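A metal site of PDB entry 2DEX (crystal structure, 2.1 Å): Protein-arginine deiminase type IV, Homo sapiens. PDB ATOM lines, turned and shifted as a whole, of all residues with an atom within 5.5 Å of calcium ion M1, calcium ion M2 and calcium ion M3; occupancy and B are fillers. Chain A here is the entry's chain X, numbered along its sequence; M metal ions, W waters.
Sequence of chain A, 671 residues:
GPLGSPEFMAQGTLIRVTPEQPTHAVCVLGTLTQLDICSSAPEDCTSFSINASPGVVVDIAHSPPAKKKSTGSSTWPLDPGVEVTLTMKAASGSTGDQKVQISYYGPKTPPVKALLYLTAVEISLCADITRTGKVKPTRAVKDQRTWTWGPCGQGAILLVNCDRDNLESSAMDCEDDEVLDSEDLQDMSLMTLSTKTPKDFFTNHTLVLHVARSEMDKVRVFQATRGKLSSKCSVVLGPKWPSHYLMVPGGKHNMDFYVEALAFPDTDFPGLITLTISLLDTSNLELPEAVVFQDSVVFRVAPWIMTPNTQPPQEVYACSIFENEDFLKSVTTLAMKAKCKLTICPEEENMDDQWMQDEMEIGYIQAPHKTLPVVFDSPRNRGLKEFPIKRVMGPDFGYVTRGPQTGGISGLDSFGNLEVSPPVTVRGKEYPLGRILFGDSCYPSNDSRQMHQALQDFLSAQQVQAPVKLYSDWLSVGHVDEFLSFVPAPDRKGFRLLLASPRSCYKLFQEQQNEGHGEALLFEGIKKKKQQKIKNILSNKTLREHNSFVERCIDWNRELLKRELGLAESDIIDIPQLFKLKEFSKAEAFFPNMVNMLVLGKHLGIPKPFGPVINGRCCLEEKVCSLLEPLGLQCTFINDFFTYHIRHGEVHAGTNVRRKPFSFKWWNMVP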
ATOM      1  N   ASN A 161      20.930 -24.952   8.045  1.00  0.00           N
ATOM      2  CA  ASN A 161      20.359 -26.218   7.645  1.00  0.00           C
ATOM      3  C   ASN A 161      21.264 -26.861   6.588  1.00  0.00           C
ATOM      4  O   ASN A 161      20.880 -27.000   5.442  1.00  0.00           O
ATOM      5  CB  ASN A 161      18.911 -26.030   7.144  1.00  0.00           C
ATOM      6  CG  ASN A 161      18.172 -27.344   6.968  1.00  0.00           C
ATOM      7  OD1 ASN A 161      18.697 -28.407   7.309  1.00  0.00           O
ATOM      8  ND2 ASN A 161      16.969 -27.274   6.399  1.00  0.00           N
ATOM      9  N   ASP A 163      22.942 -29.963   6.491  1.00  0.00           N
ATOM     10  CA  ASP A 163      23.034 -31.394   6.263  1.00  0.00           C
ATOM     11  C   ASP A 163      22.195 -31.768   5.046  1.00  0.00           C
ATOM     12  O   ASP A 163      21.779 -30.893   4.280  1.00  0.00           O
ATOM     13  CB  ASP A 163      22.644 -32.192   7.521  1.00  0.00           C
ATOM     14  CG  ASP A 163      21.180 -32.067   7.874  1.00  0.00           C
ATOM     15  OD1 ASP A 163      20.513 -31.111   7.412  1.00  0.00           O
ATOM     16  OD2 ASP A 163      20.688 -32.932   8.637  1.00  0.00           O
ATOM     17  N   ARG A 164      21.986 -33.059   4.849  1.00  0.00           N
ATOM     18  CA  ARG A 164      21.190 -33.521   3.716  1.00  0.00           C
ATOM     19  C   ARG A 164      20.321 -34.676   4.157  1.00  0.00           C
ATOM     20  O   ARG A 164      20.734 -35.817   4.085  1.00  0.00           O
ATOM     21  CB  ARG A 164      22.115 -33.962   2.577  1.00  0.00           C
ATOM     22  CG  ARG A 164      21.424 -34.546   1.365  1.00  0.00           C
ATOM     23  CD  ARG A 164      22.414 -34.761   0.237  1.00  0.00           C
ATOM     24  NE  ARG A 164      23.345 -35.872   0.496  1.00  0.00           N
ATOM     25  CZ  ARG A 164      24.679 -35.782   0.502  1.00  0.00           C
ATOM     26  NH1 ARG A 164      25.298 -34.650   0.225  1.00  0.00           N
ATOM     27  NH2 ARG A 164      25.421 -36.858   0.772  1.00  0.00           N
ATOM     28  N   ASP A 165      19.139 -34.348   4.662  1.00  0.00           N
ATOM     29  CA  ASP A 165      18.154 -35.369   4.988  1.00  0.00           C
ATOM     30  C   ASP A 165      17.491 -35.933   3.705  1.00  0.00           C
ATOM     31  O   ASP A 165      17.008 -37.068   3.711  1.00  0.00           O
ATOM     32  CB  ASP A 165      17.088 -34.809   5.931  1.00  0.00           C
ATOM     33  CG  ASP A 165      17.653 -34.360   7.249  1.00  0.00           C
ATOM     34  OD1 ASP A 165      18.361 -35.149   7.918  1.00  0.00           O
ATOM     35  OD2 ASP A 165      17.404 -33.207   7.636  1.00  0.00           O
ATOM     36  N   ASP A 173      20.189 -29.304   2.341  1.00  0.00           N
ATOM     37  CA  ASP A 173      18.734 -29.080   2.391  1.00  0.00           C
ATOM     38  C   ASP A 173      18.331 -27.599   2.225  1.00  0.00           C
ATOM     39  O   ASP A 173      17.308 -27.311   1.626  1.00  0.00           O
ATOM     40  CB  ASP A 173      18.145 -29.634   3.707  1.00  0.00           C
ATOM     41  CG  ASP A 173      18.244 -31.152   3.832  1.00  0.00           C
ATOM     42  OD1 ASP A 173      18.182 -31.905   2.820  1.00  0.00           O
ATOM     43  OD2 ASP A 173      18.339 -31.594   4.989  1.00  0.00           O
ATOM     44  N   CYS A 174      19.139 -26.654   2.740  1.00  0.00           N
ATOM     45  CA  CYS A 174      18.790 -25.218   2.694  1.00  0.00           C
ATOM     46  C   CYS A 174      18.993 -24.551   1.325  1.00  0.00           C
ATOM     47  O   CYS A 174      18.678 -23.364   1.168  1.00  0.00           O
ATOM     48  CB  CYS A 174      19.611 -24.446   3.725  1.00  0.00           C
ATOM     49  SG  CYS A 174      21.354 -24.536   3.350  1.00  0.00           S
ATOM     50  N   GLU A 175      19.527 -25.283   0.339  1.00  0.00           N
ATOM     51  CA  GLU A 175      19.745 -24.749  -1.025  1.00  0.00           C
ATOM     52  C   GLU A 175      18.491 -24.490  -1.892  1.00  0.00           C
ATOM     53  O   GLU A 175      18.519 -23.631  -2.782  1.00  0.00           O
ATOM     54  CB  GLU A 175      20.718 -25.647  -1.817  1.00  0.00           C
ATOM     55  CG  GLU A 175      22.194 -25.529  -1.358  1.00  0.00           C
ATOM     56  CD  GLU A 175      23.097 -26.611  -1.953  1.00  0.00           C
ATOM     57  OE1 GLU A 175      22.940 -26.936  -3.161  1.00  0.00           O
ATOM     58  OE2 GLU A 175      23.958 -27.148  -1.208  1.00  0.00           O
ATOM     59  N   ASP A 176      17.396 -25.224  -1.666  1.00  0.00           N
ATOM     60  CA  ASP A 176      16.128 -24.980  -2.401  1.00  0.00           C
ATOM     61  C   ASP A 176      15.157 -24.244  -1.501  1.00  0.00           C
ATOM     62  O   ASP A 176      15.490 -23.925  -0.349  1.00  0.00           O
ATOM     63  CB  ASP A 176      15.504 -26.307  -2.859  1.00  0.00           C
ATOM     64  CG  ASP A 176      15.101 -27.213  -1.691  1.00  0.00           C
ATOM     65  OD1 ASP A 176      15.215 -26.753  -0.512  1.00  0.00           O
ATOM     66  OD2 ASP A 176      14.698 -28.372  -1.929  1.00  0.00           O
ATOM     67  N   ASP A 177      13.961 -23.975  -2.000  1.00  0.00           N
ATOM     68  CA  ASP A 177      12.897 -23.327  -1.189  1.00  0.00           C
ATOM     69  C   ASP A 177      11.709 -24.262  -0.959  1.00  0.00           C
ATOM     70  O   ASP A 177      10.546 -23.874  -1.136  1.00  0.00           O
ATOM     71  CB  ASP A 177      12.447 -21.985  -1.777  1.00  0.00           C
ATOM     72  CG  ASP A 177      12.667 -21.888  -3.264  1.00  0.00           C
ATOM     73  OD1 ASP A 177      11.815 -22.390  -4.054  1.00  0.00           O
ATOM     74  OD2 ASP A 177      13.726 -21.326  -3.635  1.00  0.00           O
ATOM     75  N   GLU A 178      12.027 -25.496  -0.564  1.00  0.00           N
ATOM     76  CA  GLU A 178      11.013 -26.468  -0.185  1.00  0.00           C
ATOM     77  C   GLU A 178      11.458 -27.262   1.019  1.00  0.00           C
ATOM     78  O   GLU A 178      12.648 -27.491   1.200  1.00  0.00           O
ATOM     79  CB  GLU A 178      10.767 -27.434  -1.329  1.00  0.00           C
ATOM     80  CG  GLU A 178      10.450 -26.745  -2.622  1.00  0.00           C
ATOM     81  CD  GLU A 178       9.894 -27.683  -3.663  1.00  0.00           C
ATOM     82  OE1 GLU A 178       9.057 -28.526  -3.294  1.00  0.00           O
ATOM     83  OE2 GLU A 178      10.300 -27.568  -4.834  1.00  0.00           O
ATOM     84  N   VAL A 179      10.514 -27.680   1.847  1.00  0.00           N
ATOM     85  CA  VAL A 179      10.780 -28.705   2.850  1.00  0.00           C
ATOM     86  C   VAL A 179      10.411 -30.024   2.169  1.00  0.00           C
ATOM     87  O   VAL A 179       9.243 -30.247   1.847  1.00  0.00           O
ATOM     88  CB  VAL A 179       9.935 -28.513   4.123  1.00  0.00           C
ATOM     89  CG1 VAL A 179      10.338 -29.518   5.195  1.00  0.00           C
ATOM     90  CG2 VAL A 179      10.096 -27.113   4.647  1.00  0.00           C
ATOM     91  N   LEU A 180      11.411 -30.862   1.908  1.00  0.00           N
ATOM     92  CA  LEU A 180      11.207 -32.072   1.107  1.00  0.00           C
ATOM     93  C   LEU A 180      11.036 -33.333   1.950  1.00  0.00           C
ATOM     94  O   LEU A 180      10.645 -34.371   1.417  1.00  0.00           O
ATOM     95  CB  LEU A 180      12.367 -32.273   0.122  1.00  0.00           C
ATOM     96  CG  LEU A 180      12.355 -31.308  -1.065  1.00  0.00           C
ATOM     97  CD1 LEU A 180      13.577 -31.564  -1.918  1.00  0.00           C
ATOM     98  CD2 LEU A 180      11.073 -31.436  -1.891  1.00  0.00           C
ATOM     99  N   GLU A 183      11.426 -34.937   8.406  1.00  0.00           N
ATOM    100  CA  GLU A 183      12.522 -34.903   9.379  1.00  0.00           C
ATOM    101  C   GLU A 183      13.453 -33.698   9.209  1.00  0.00           C
ATOM    102  O   GLU A 183      14.164 -33.347  10.136  1.00  0.00           O
ATOM    103  CB  GLU A 183      13.342 -36.218   9.388  1.00  0.00           C
ATOM    104  CG  GLU A 183      13.518 -36.943   8.029  1.00  0.00           C
ATOM    105  CD  GLU A 183      12.295 -37.748   7.596  1.00  0.00           C
ATOM    106  OE1 GLU A 183      11.566 -38.290   8.466  1.00  0.00           O
ATOM    107  OE2 GLU A 183      12.065 -37.833   6.376  1.00  0.00           O
ATOM    108  N   ASP A 184      13.449 -33.086   8.041  1.00  0.00           N
ATOM    109  CA  ASP A 184      14.168 -31.841   7.810  1.00  0.00           C
ATOM    110  C   ASP A 184      13.689 -30.779   8.814  1.00  0.00           C
ATOM    111  O   ASP A 184      14.513 -30.015   9.361  1.00  0.00           O
ATOM    112  CB  ASP A 184      13.952 -31.351   6.375  1.00  0.00           C
ATOM    113  CG  ASP A 184      14.837 -30.170   6.013  1.00  0.00           C
ATOM    114  OD1 ASP A 184      16.021 -30.160   6.450  1.00  0.00           O
ATOM    115  OD2 ASP A 184      14.360 -29.273   5.290  1.00  0.00           O
ATOM    116  N   ASP A 187      15.401 -29.941  12.079  1.00  0.00           N
ATOM    117  CA  ASP A 187      16.570 -29.083  12.078  1.00  0.00           C
ATOM    118  C   ASP A 187      16.166 -27.633  12.208  1.00  0.00           C
ATOM    119  O   ASP A 187      16.992 -26.815  12.588  1.00  0.00           O
ATOM    120  CB  ASP A 187      17.370 -29.230  10.786  1.00  0.00           C
ATOM    121  CG  ASP A 187      17.948 -30.605  10.611  1.00  0.00           C
ATOM    122  OD1 ASP A 187      18.265 -31.260  11.628  1.00  0.00           O
ATOM    123  OD2 ASP A 187      18.069 -31.031   9.447  1.00  0.00           O
ATOM    124  N   MET A 188      14.919 -27.321  11.871  1.00  0.00           N
ATOM    125  CA  MET A 188      14.446 -25.934  11.801  1.00  0.00           C
ATOM    126  C   MET A 188      13.895 -25.429  13.124  1.00  0.00           C
ATOM    127  O   MET A 188      13.535 -26.199  13.987  1.00  0.00           O
ATOM    128  CB  MET A 188      13.386 -25.832  10.715  1.00  0.00           C
ATOM    129  CG  MET A 188      13.911 -26.236   9.359  1.00  0.00           C
ATOM    130  SD  MET A 188      12.714 -25.916   8.056  1.00  0.00           S
ATOM    131  CE  MET A 188      13.425 -26.807   6.718  1.00  0.00           C
ATOM    132  N   PHE A 222       9.244 -20.956   6.430  1.00  0.00           N
ATOM    133  CA  PHE A 222       8.124 -21.746   5.873  1.00  0.00           C
ATOM    134  C   PHE A 222       6.909 -21.657   6.774  1.00  0.00           C
ATOM    135  O   PHE A 222       7.025 -21.680   7.997  1.00  0.00           O
ATOM    136  CB  PHE A 222       8.491 -23.239   5.765  1.00  0.00           C
ATOM    137  CG  PHE A 222       9.608 -23.534   4.807  1.00  0.00           C
ATOM    138  CD1 PHE A 222      10.919 -23.560   5.239  1.00  0.00           C
ATOM    139  CD2 PHE A 222       9.328 -23.807   3.462  1.00  0.00           C
ATOM    140  CE1 PHE A 222      11.951 -23.826   4.362  1.00  0.00           C
ATOM    141  CE2 PHE A 222      10.360 -24.085   2.567  1.00  0.00           C
ATOM    142  CZ  PHE A 222      11.672 -24.078   3.025  1.00  0.00           C
ATOM    143  N   GLU A 260      14.863 -21.817   8.855  1.00  0.00           N
ATOM    144  CA  GLU A 260      16.201 -22.408   8.635  1.00  0.00           C
ATOM    145  C   GLU A 260      17.155 -21.267   8.363  1.00  0.00           C
ATOM    146  O   GLU A 260      16.771 -20.271   7.727  1.00  0.00           O
ATOM    147  CB  GLU A 260      16.182 -23.444   7.476  1.00  0.00           C
ATOM    148  CG  GLU A 260      15.745 -22.878   6.127  1.00  0.00           C
ATOM    149  CD  GLU A 260      15.770 -23.868   4.977  1.00  0.00           C
ATOM    150  OE1 GLU A 260      16.071 -25.072   5.154  1.00  0.00           O
ATOM    151  OE2 GLU A 260      15.468 -23.438   3.855  1.00  0.00           O
ATOM    152  N   LYS A 370      18.012 -29.439  18.632  1.00  0.00           N
ATOM    153  CA  LYS A 370      18.765 -30.300  17.739  1.00  0.00           C
ATOM    154  C   LYS A 370      20.270 -29.993  17.796  1.00  0.00           C
ATOM    155  O   LYS A 370      20.678 -28.842  17.862  1.00  0.00           O
ATOM    156  CB  LYS A 370      18.230 -30.147  16.296  1.00  0.00           C
ATOM    157  CG  LYS A 370      19.043 -30.903  15.214  1.00  0.00           C
ATOM    158  CD  LYS A 370      18.868 -32.450  15.320  1.00  0.00           C
ATOM    159  CE  LYS A 370      17.863 -32.965  14.307  1.00  0.00           C
ATOM    160  NZ  LYS A 370      17.286 -34.299  14.641  1.00  0.00           N
ATOM    161  N   LEU A 372      23.802 -31.477  15.721  1.00  0.00           N
ATOM    162  CA  LEU A 372      24.306 -32.410  14.704  1.00  0.00           C
ATOM    163  C   LEU A 372      25.768 -32.177  14.382  1.00  0.00           C
ATOM    164  O   LEU A 372      26.257 -31.061  14.499  1.00  0.00           O
ATOM    165  CB  LEU A 372      23.494 -32.350  13.410  1.00  0.00           C
ATOM    166  CG  LEU A 372      23.329 -31.028  12.665  1.00  0.00           C
ATOM    167  CD1 LEU A 372      23.298 -31.218  11.140  1.00  0.00           C
ATOM    168  CD2 LEU A 372      22.070 -30.363  13.106  1.00  0.00           C
ATOM    169  N   PRO A 395      22.336 -37.445   5.958  1.00  0.00           N
ATOM    170  CA  PRO A 395      21.315 -37.226   6.982  1.00  0.00           C
ATOM    171  C   PRO A 395      21.922 -36.968   8.375  1.00  0.00           C
ATOM    172  O   PRO A 395      22.705 -37.775   8.861  1.00  0.00           O
ATOM    173  CB  PRO A 395      20.501 -38.536   6.961  1.00  0.00           C
ATOM    174  CG  PRO A 395      20.685 -39.055   5.550  1.00  0.00           C
ATOM    175  CD  PRO A 395      22.152 -38.737   5.269  1.00  0.00           C
ATOM    176  N   ASP A 396      21.562 -35.831   8.967  1.00  0.00           N
ATOM    177  CA  ASP A 396      22.108 -35.382  10.274  1.00  0.00           C
ATOM    178  C   ASP A 396      23.639 -35.280  10.335  1.00  0.00           C
ATOM    179  O   ASP A 396      24.260 -35.361  11.393  1.00  0.00           O
ATOM    180  CB  ASP A 396      21.513 -36.194  11.436  1.00  0.00           C
ATOM    181  CG  ASP A 396      20.075 -35.771  11.768  1.00  0.00           C
ATOM    182  OD1 ASP A 396      19.706 -34.609  11.499  1.00  0.00           O
ATOM    183  OD2 ASP A 396      19.317 -36.599  12.273  1.00  0.00           O
HETATM  184 CA    CA M   1      14.899 -27.476   1.572  1.00  0.00          CA
HETATM  185 CA    CA M   2      18.093 -30.829   7.155  1.00  0.00          CA
HETATM  186 CA    CA M   3      18.571 -33.332   9.934  1.00  0.00          CA
HETATM  187  O   HOH W   1      14.959 -25.116   1.961  1.00  0.00           O
HETATM  188  O   HOH W   2      16.458 -34.152  10.571  1.00  0.00           O
HETATM  189  O   HOH W   3      15.213 -27.010   3.766  1.00  0.00           O
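Calcium ion M2 is bound by OD1 of Asp 184, OD2 of Asp 187, OD2 of Asp 173, OD1 of Asp 163, OD1 of Asn 161 and OD2 of Asp 165.
Calcium ion M2 has six donor atoms within binding distance.
Four residues have an atom within 4 Å of calcium ion M3: Asp 163, Asp 165, Asp 187 and Asp 396.
The nearest printed residue that does not touch calcium ion M3 is Glu 183 (4.4 Å).
OD1 of Asp 396 is bound to calcium ion M3 (2.3 Å).
Water W2 binds calcium ion M3.
The side-chain carboxylate (OD2) of Asp 187 binds calcium ion M3.
Calcium ion M3 is bound by OD2 of Asp 163 (2.5 Å).
OD2 of Asp 165 is bound to calcium ion M3 (2.6 Å).
OD1 of Asp 187 binds calcium ion M3 (2.7 Å).
Calcium ion M3 is bound by OD1 of Asp 165, 2.7 Å away.
OD2 of Asp 396 lies within salt-bridge range of NZ of Lys 370, at 3.9 Å.
OE1 of Glu 260 sits at hydrogen-bond distance from ND2 of Asn 161 (2.7 Å).
O of Asn 161 lies within hydrogen-bond range of N of Cys 174 (3.2 Å).
The nearest printed residue that does not touch calcium ion M1 is Asp 184 (4.2 Å).
OD1 of Asp 176 binds calcium ion M1.
Calcium ion M1 is bound by water W3.
Calcium ion M1 is bound by O of Glu 178.
Calcium ion M1 is bound by water W1, 2.4 Å away.
Calcium ion M1 is bound by the backbone carbonyl oxygen (O) of Asp 173 (2.4 Å).
Six residues have an atom within 4 Å of calcium ion M2: Asn 161, Asp 163, Asp 165, Asp 173, Asp 184 and Asp 187.
Along chain A the residues within 4 Å of calcium ion M2 span positions 161 to 187.
Water W1 bridges OE2 of Glu 260 (2.6 Å) and O of Asp 176 (2.7 Å).
Water W3 lies within hydrogen-bond range of OE1 of Glu 260, OD2 of Asp 184 and ND2 of Asn 161.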
